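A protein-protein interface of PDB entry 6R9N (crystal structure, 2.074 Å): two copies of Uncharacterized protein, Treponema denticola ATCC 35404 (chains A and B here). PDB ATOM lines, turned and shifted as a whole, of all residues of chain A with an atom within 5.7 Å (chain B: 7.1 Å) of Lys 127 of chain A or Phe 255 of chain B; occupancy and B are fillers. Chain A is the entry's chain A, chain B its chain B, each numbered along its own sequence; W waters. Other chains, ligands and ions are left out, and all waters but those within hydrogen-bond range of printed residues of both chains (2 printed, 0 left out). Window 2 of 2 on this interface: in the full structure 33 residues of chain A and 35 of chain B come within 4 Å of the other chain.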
ATOM      1  N   PRO A 125     -10.924  31.276 -18.045  1.00  0.00           N
ATOM      2  CA  PRO A 125     -11.632  31.522 -16.787  1.00  0.00           C
ATOM      3  C   PRO A 125     -10.710  31.244 -15.618  1.00  0.00           C
ATOM      4  O   PRO A 125      -9.693  30.563 -15.750  1.00  0.00           O
ATOM      5  CB  PRO A 125     -12.805  30.536 -16.832  1.00  0.00           C
ATOM      6  CG  PRO A 125     -12.284  29.396 -17.677  1.00  0.00           C
ATOM      7  CD  PRO A 125     -11.305  29.993 -18.670  1.00  0.00           C
ATOM      8  N   ASP A 126     -11.101  31.748 -14.449  1.00  0.00           N
ATOM      9  CA  ASP A 126     -10.175  31.802 -13.318  1.00  0.00           C
ATOM     10  C   ASP A 126      -9.563  30.443 -12.961  1.00  0.00           C
ATOM     11  O   ASP A 126      -8.407  30.393 -12.529  1.00  0.00           O
ATOM     12  CB  ASP A 126     -10.885  32.401 -12.101  1.00  0.00           C
ATOM     13  CG  ASP A 126     -10.934  33.916 -12.159  1.00  0.00           C
ATOM     14  OD1 ASP A 126     -10.203  34.508 -12.993  1.00  0.00           O
ATOM     15  OD2 ASP A 126     -11.703  34.517 -11.386  1.00  0.00           O
ATOM     16  N   LYS A 127     -10.293  29.337 -13.122  1.00  0.00           N
ATOM     17  CA  LYS A 127      -9.781  28.031 -12.711  1.00  0.00           C
ATOM     18  C   LYS A 127      -9.072  27.279 -13.837  1.00  0.00           C
ATOM     19  O   LYS A 127      -8.679  26.122 -13.651  1.00  0.00           O
ATOM     20  CB  LYS A 127     -10.904  27.162 -12.140  1.00  0.00           C
ATOM     21  CG  LYS A 127     -11.371  27.621 -10.763  1.00  0.00           C
ATOM     22  CD  LYS A 127     -12.545  26.821 -10.246  1.00  0.00           C
ATOM     23  CE  LYS A 127     -13.163  27.524  -9.046  1.00  0.00           C
ATOM     24  NZ  LYS A 127     -13.515  26.578  -7.965  1.00  0.00           N
ATOM     25  N   GLY A 128      -8.883  27.911 -14.984  1.00  0.00           N
ATOM     26  CA  GLY A 128      -8.092  27.346 -16.049  1.00  0.00           C
ATOM     27  C   GLY A 128      -8.957  26.623 -17.050  1.00  0.00           C
ATOM     28  O   GLY A 128     -10.182  26.556 -16.937  1.00  0.00           O
ATOM     29  N   MET A 129      -8.279  26.086 -18.056  1.00  0.00           N
ATOM     30  CA  MET A 129      -8.904  25.331 -19.131  1.00  0.00           C
ATOM     31  C   MET A 129      -7.802  24.521 -19.800  1.00  0.00           C
ATOM     32  O   MET A 129      -6.614  24.758 -19.579  1.00  0.00           O
ATOM     33  CB  MET A 129      -9.598  26.256 -20.130  1.00  0.00           C
ATOM     34  CG  MET A 129      -8.615  27.143 -20.901  1.00  0.00           C
ATOM     35  SD  MET A 129      -9.349  28.406 -21.951  1.00  0.00           S
ATOM     36  CE  MET A 129     -10.611  27.469 -22.815  1.00  0.00           C
ATOM     37  N   CYS A 141      -3.976  25.155 -18.658  1.00  0.00           N
ATOM     38  CA  CYS A 141      -3.724  26.492 -18.137  1.00  0.00           C
ATOM     39  C   CYS A 141      -3.803  26.426 -16.617  1.00  0.00           C
ATOM     40  O   CYS A 141      -4.836  26.042 -16.066  1.00  0.00           O
ATOM     41  CB  CYS A 141      -4.760  27.481 -18.675  1.00  0.00           C
ATOM     42  SG  CYS A 141      -4.686  27.802 -20.485  1.00  0.00           S
ATOM     43  N   PRO A 143      -3.832  27.960 -12.931  1.00  0.00           N
ATOM     44  CA  PRO A 143      -4.105  29.199 -12.193  1.00  0.00           C
ATOM     45  C   PRO A 143      -2.888  29.646 -11.398  1.00  0.00           C
ATOM     46  O   PRO A 143      -2.342  28.893 -10.588  1.00  0.00           O
ATOM     47  CB  PRO A 143      -5.266  28.808 -11.267  1.00  0.00           C
ATOM     48  CG  PRO A 143      -5.871  27.594 -11.885  1.00  0.00           C
ATOM     49  CD  PRO A 143      -4.751  26.871 -12.555  1.00  0.00           C
ATOM     50  N   SER A 144      -2.489  30.900 -11.594  1.00  0.00           N
ATOM     51  CA  SER A 144      -1.295  31.429 -10.933  1.00  0.00           C
ATOM     52  C   SER A 144      -1.544  32.853 -10.504  1.00  0.00           C
ATOM     53  O   SER A 144      -0.672  33.721 -10.626  1.00  0.00           O
ATOM     54  CB  SER A 144      -0.075  31.349 -11.852  1.00  0.00           C
ATOM     55  OG  SER A 144       0.113  30.022 -12.314  1.00  0.00           O
ATOM     56  N   HIS A 145      -2.746  33.107  -9.999  1.00  0.00           N
ATOM     57  CA  HIS A 145      -3.210  34.463  -9.789  1.00  0.00           C
ATOM     58  C   HIS A 145      -2.488  35.118  -8.614  1.00  0.00           C
ATOM     59  O   HIS A 145      -2.073  34.460  -7.655  1.00  0.00           O
ATOM     60  CB  HIS A 145      -4.728  34.457  -9.581  1.00  0.00           C
ATOM     61  CG  HIS A 145      -5.472  33.769 -10.682  1.00  0.00           C
ATOM     62  ND1 HIS A 145      -5.424  34.199 -11.993  1.00  0.00           N
ATOM     63  CD2 HIS A 145      -6.265  32.671 -10.673  1.00  0.00           C
ATOM     64  CE1 HIS A 145      -6.165  33.399 -12.742  1.00  0.00           C
ATOM     65  NE2 HIS A 145      -6.683  32.461 -11.965  1.00  0.00           N
ATOM     66  N   PHE A 153      -1.819  32.861 -15.730  1.00  0.00           N
ATOM     67  CA  PHE A 153      -1.780  31.410 -15.847  1.00  0.00           C
ATOM     68  C   PHE A 153      -0.396  30.938 -16.268  1.00  0.00           C
ATOM     69  O   PHE A 153       0.324  31.614 -17.010  1.00  0.00           O
ATOM     70  CB  PHE A 153      -2.830  30.877 -16.858  1.00  0.00           C
ATOM     71  CG  PHE A 153      -4.233  31.101 -16.422  1.00  0.00           C
ATOM     72  CD1 PHE A 153      -4.893  30.147 -15.657  1.00  0.00           C
ATOM     73  CD2 PHE A 153      -4.891  32.282 -16.736  1.00  0.00           C
ATOM     74  CE1 PHE A 153      -6.191  30.357 -15.234  1.00  0.00           C
ATOM     75  CE2 PHE A 153      -6.191  32.502 -16.302  1.00  0.00           C
ATOM     76  CZ  PHE A 153      -6.834  31.544 -15.548  1.00  0.00           C
ATOM     77  N   ILE A 205      -1.050  32.782  -0.898  1.00  0.00           N
ATOM     78  CA  ILE A 205      -1.272  32.424  -2.298  1.00  0.00           C
ATOM     79  C   ILE A 205      -0.141  31.533  -2.794  1.00  0.00           C
ATOM     80  O   ILE A 205      -0.367  30.547  -3.511  1.00  0.00           O
ATOM     81  CB  ILE A 205      -1.447  33.679  -3.178  1.00  0.00           C
ATOM     82  CG1 ILE A 205      -1.965  33.276  -4.551  1.00  0.00           C
ATOM     83  CG2 ILE A 205      -0.142  34.451  -3.325  1.00  0.00           C
ATOM     84  CD1 ILE A 205      -3.319  32.534  -4.494  1.00  0.00           C
ATOM     85  N   LYS A 208      -0.478  27.736  -1.605  1.00  0.00           N
ATOM     86  CA  LYS A 208      -1.545  27.035  -2.317  1.00  0.00           C
ATOM     87  C   LYS A 208      -1.119  26.682  -3.742  1.00  0.00           C
ATOM     88  O   LYS A 208      -1.422  25.590  -4.241  1.00  0.00           O
ATOM     89  CB  LYS A 208      -2.816  27.887  -2.344  1.00  0.00           C
ATOM     90  CG  LYS A 208      -4.027  27.170  -2.958  1.00  0.00           C
ATOM     91  N   TRP A 209      -0.434  27.607  -4.421  1.00  0.00           N
ATOM     92  CA  TRP A 209       0.086  27.325  -5.757  1.00  0.00           C
ATOM     93  C   TRP A 209       1.027  26.128  -5.733  1.00  0.00           C
ATOM     94  O   TRP A 209       0.894  25.208  -6.542  1.00  0.00           O
ATOM     95  CB  TRP A 209       0.806  28.556  -6.309  1.00  0.00           C
ATOM     96  CG  TRP A 209       1.186  28.449  -7.780  1.00  0.00           C
ATOM     97  CD1 TRP A 209       0.390  28.740  -8.858  1.00  0.00           C
ATOM     98  CD2 TRP A 209       2.448  28.045  -8.313  1.00  0.00           C
ATOM     99  NE1 TRP A 209       1.080  28.544 -10.024  1.00  0.00           N
ATOM    100  CE2 TRP A 209       2.345  28.107  -9.721  1.00  0.00           C
ATOM    101  CE3 TRP A 209       3.652  27.617  -7.741  1.00  0.00           C
ATOM    102  CZ2 TRP A 209       3.399  27.772 -10.557  1.00  0.00           C
ATOM    103  CZ3 TRP A 209       4.697  27.296  -8.576  1.00  0.00           C
ATOM    104  CH2 TRP A 209       4.566  27.374  -9.969  1.00  0.00           C
ATOM    105  N   TYR A 212      -0.848  22.948  -5.444  1.00  0.00           N
ATOM    106  CA  TYR A 212      -1.489  22.650  -6.721  1.00  0.00           C
ATOM    107  C   TYR A 212      -0.477  22.094  -7.710  1.00  0.00           C
ATOM    108  O   TYR A 212      -0.693  21.036  -8.320  1.00  0.00           O
ATOM    109  CB  TYR A 212      -2.149  23.926  -7.261  1.00  0.00           C
ATOM    110  CG  TYR A 212      -3.075  23.775  -8.455  1.00  0.00           C
ATOM    111  CD1 TYR A 212      -2.573  23.535  -9.727  1.00  0.00           C
ATOM    112  CD2 TYR A 212      -4.453  23.917  -8.312  1.00  0.00           C
ATOM    113  CE1 TYR A 212      -3.417  23.408 -10.828  1.00  0.00           C
ATOM    114  CE2 TYR A 212      -5.310  23.802  -9.405  1.00  0.00           C
ATOM    115  CZ  TYR A 212      -4.778  23.553 -10.662  1.00  0.00           C
ATOM    116  OH  TYR A 212      -5.602  23.437 -11.757  1.00  0.00           O
ATOM    117  N   TYR B 250     -11.052  35.094  -1.375  1.00  0.00           N
ATOM    118  CA  TYR B 250     -11.891  34.087  -2.029  1.00  0.00           C
ATOM    119  C   TYR B 250     -11.013  33.097  -2.777  1.00  0.00           C
ATOM    120  O   TYR B 250     -11.176  32.891  -3.986  1.00  0.00           O
ATOM    121  CB  TYR B 250     -12.877  34.738  -2.994  1.00  0.00           C
ATOM    122  CG  TYR B 250     -13.951  35.555  -2.319  1.00  0.00           C
ATOM    123  CD1 TYR B 250     -14.970  34.943  -1.611  1.00  0.00           C
ATOM    124  CD2 TYR B 250     -13.941  36.940  -2.389  1.00  0.00           C
ATOM    125  CE1 TYR B 250     -15.959  35.695  -0.989  1.00  0.00           C
ATOM    126  CE2 TYR B 250     -14.917  37.702  -1.766  1.00  0.00           C
ATOM    127  CZ  TYR B 250     -15.928  37.070  -1.071  1.00  0.00           C
ATOM    128  OH  TYR B 250     -16.915  37.811  -0.454  1.00  0.00           O
ATOM    129  N   ILE B 251     -10.047  32.508  -2.070  1.00  0.00           N
ATOM    130  CA  ILE B 251      -9.025  31.721  -2.738  1.00  0.00           C
ATOM    131  C   ILE B 251      -9.589  30.448  -3.366  1.00  0.00           C
ATOM    132  O   ILE B 251      -9.020  29.940  -4.340  1.00  0.00           O
ATOM    133  CB  ILE B 251      -7.896  31.403  -1.748  1.00  0.00           C
ATOM    134  CG1 ILE B 251      -6.669  30.881  -2.503  1.00  0.00           C
ATOM    135  CG2 ILE B 251      -8.394  30.427  -0.689  1.00  0.00           C
ATOM    136  CD1 ILE B 251      -5.405  30.836  -1.660  1.00  0.00           C
ATOM    137  N   GLU B 252     -10.719  29.937  -2.872  1.00  0.00           N
ATOM    138  CA  GLU B 252     -11.296  28.756  -3.505  1.00  0.00           C
ATOM    139  C   GLU B 252     -11.792  29.058  -4.915  1.00  0.00           C
ATOM    140  O   GLU B 252     -11.885  28.143  -5.746  1.00  0.00           O
ATOM    141  CB  GLU B 252     -12.436  28.200  -2.650  1.00  0.00           C
ATOM    142  CG  GLU B 252     -13.691  29.094  -2.623  1.00  0.00           C
ATOM    143  CD  GLU B 252     -13.575  30.278  -1.650  1.00  0.00           C
ATOM    144  OE1 GLU B 252     -12.522  30.416  -0.987  1.00  0.00           O
ATOM    145  OE2 GLU B 252     -14.552  31.066  -1.523  1.00  0.00           O
ATOM    146  N   ASN B 253     -12.072  30.324  -5.222  1.00  0.00           N
ATOM    147  CA  ASN B 253     -12.406  30.684  -6.590  1.00  0.00           C
ATOM    148  C   ASN B 253     -11.190  30.741  -7.508  1.00  0.00           C
ATOM    149  O   ASN B 253     -11.368  30.817  -8.726  1.00  0.00           O
ATOM    150  CB  ASN B 253     -13.108  32.042  -6.622  1.00  0.00           C
ATOM    151  CG  ASN B 253     -14.405  32.044  -5.857  1.00  0.00           C
ATOM    152  OD1 ASN B 253     -14.921  30.992  -5.497  1.00  0.00           O
ATOM    153  ND2 ASN B 253     -14.953  33.234  -5.617  1.00  0.00           N
ATOM    154  N   LEU B 254      -9.972  30.736  -6.968  1.00  0.00           N
ATOM    155  CA  LEU B 254      -8.769  30.938  -7.778  1.00  0.00           C
ATOM    156  C   LEU B 254      -8.071  29.639  -8.168  1.00  0.00           C
ATOM    157  O   LEU B 254      -7.078  29.685  -8.897  1.00  0.00           O
ATOM    158  CB  LEU B 254      -7.771  31.838  -7.036  1.00  0.00           C
ATOM    159  CG  LEU B 254      -8.254  33.197  -6.507  1.00  0.00           C
ATOM    160  CD1 LEU B 254      -7.130  33.903  -5.751  1.00  0.00           C
ATOM    161  CD2 LEU B 254      -8.780  34.107  -7.624  1.00  0.00           C
ATOM    162  N   PHE B 255      -8.561  28.493  -7.703  1.00  0.00           N
ATOM    163  CA  PHE B 255      -8.021  27.196  -8.073  1.00  0.00           C
ATOM    164  C   PHE B 255      -9.174  26.220  -8.287  1.00  0.00           C
ATOM    165  O   PHE B 255      -9.102  25.363  -9.175  1.00  0.00           O
ATOM    166  CB  PHE B 255      -7.065  26.664  -6.993  1.00  0.00           C
ATOM    167  CG  PHE B 255      -5.841  27.524  -6.776  1.00  0.00           C
ATOM    168  CD1 PHE B 255      -4.667  27.290  -7.494  1.00  0.00           C
ATOM    169  CD2 PHE B 255      -5.856  28.555  -5.847  1.00  0.00           C
ATOM    170  CE1 PHE B 255      -3.533  28.079  -7.295  1.00  0.00           C
ATOM    171  CE2 PHE B 255      -4.728  29.348  -5.640  1.00  0.00           C
ATOM    172  CZ  PHE B 255      -3.561  29.107  -6.372  1.00  0.00           C
HETATM  173  O   HOH W   1      -7.852  24.418 -11.571  1.00  0.00           O
HETATM  174  O   HOH W   2      -4.269  31.119  -8.810  1.00  0.00           O
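No position is printed for both chains.
Of the 14 pairs that touch across the chains among the printed residues, none has its exchanged pair printed and touching as well.
Water W1 lies within hydrogen-bond range of OH of Tyr 212 of chain A (2.5 Å), O of Lys 127 of chain A (2.8 Å) and O of Phe 255 of chain B (2.9 Å).
Water W2 lies within hydrogen-bond range of N of His 145 of chain A, O of Leu 254 of chain B, N of Ser 144 of chain A and O of Pro 143 of chain A.
The backbone carbonyl oxygen (O) of Glu 252 of chain B lies within hydrogen-bond range of the side-chain amino group (NZ) of Lys 127 of chain A.
O of Pro 143 of chain A lies close to NE1 of Trp 209 of chain A (3.5 Å).
O of Asp 126 of chain A is in hydrogen-bond range of NE2 of His 145 of chain A, 2.8 Å away.
The side-chain hydroxyl (OG) of Ser 144 of chain A lies within hydrogen-bond range of the indole nitrogen (NE1) of Trp 209 of chain A, 2.9 Å away.
Phe 255 of chain B touches just these residues of chain A: Lys 127 (3.6 Å), Pro 143 (3.6 Å), Ile 205 (3.7 Å), Lys 208 (3.5 Å), Trp 209 (3.98 Å) and Tyr 212 (3.5 Å).
Of the printed residues of chain A, Asn 253 of chain B touches Asp 126 and Lys 127.
Of the printed residues of chain B, Asp 126 of chain A touches Asn 253 and Leu 254.
Of the printed residues of chain B, Lys 208 of chain A touches Ile 251 (3.98 Å) and Phe 255 (3.5 Å).
Of the printed residues of chain B, Pro 143 of chain A touches Leu 254 (3.1 Å) and Phe 255 (3.6 Å).
Of the printed residues of chain B, Tyr 212 of chain A touches Phe 255.
Met 129 of chain A touches none of the printed residues of chain B.
The nearest residue of chain A that does not touch Phe 255 of chain B is Asp 126 of chain A (5.2 Å).
The nearest printed residue of chain A that does not touch Asn 253 of chain B is His 145 of chain A (5.8 Å).
Asp 126 of chain A touches Leu 254 of chain B.
Asn 253 of chain B touches Lys 127 of chain A.
Lys 127 of chain A touches Phe 255 of chain B.
Pro 143 of chain A touches Phe 255 of chain B.
Leu 254 of chain B touches His 145 of chain A.
Ile 205 of chain A touches Ile 251 of chain B.
Ile 205 of chain A touches Phe 255 of chain B (CD1 to CE2, 3.7 Å).
Lys 208 of chain A touches Phe 255 of chain B.
CZ of Phe 255 of chain B touches N of Trp 209 of chain A (3.98 Å).
CD1 of Phe 255 of chain B touches CD2 of Tyr 212 of chain A, 3.5 Å away.
Of the 6 printed residues of chain B, 5 touch a printed residue of chain A.
Printed residues of chain B that touch a printed residue of chain A: Ile 251, Glu 252, Asn 253, Leu 254 and Phe 255.
Along chain A the printed residues that touch a printed residue of chain B span positions 126 to 212.
Among the printed residues, 14 pairs touch across the chains.
Among the printed residues, no Asp or Glu carboxylate lies within 4 Å of a Lys or Arg side-chain nitrogen of the other chain.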
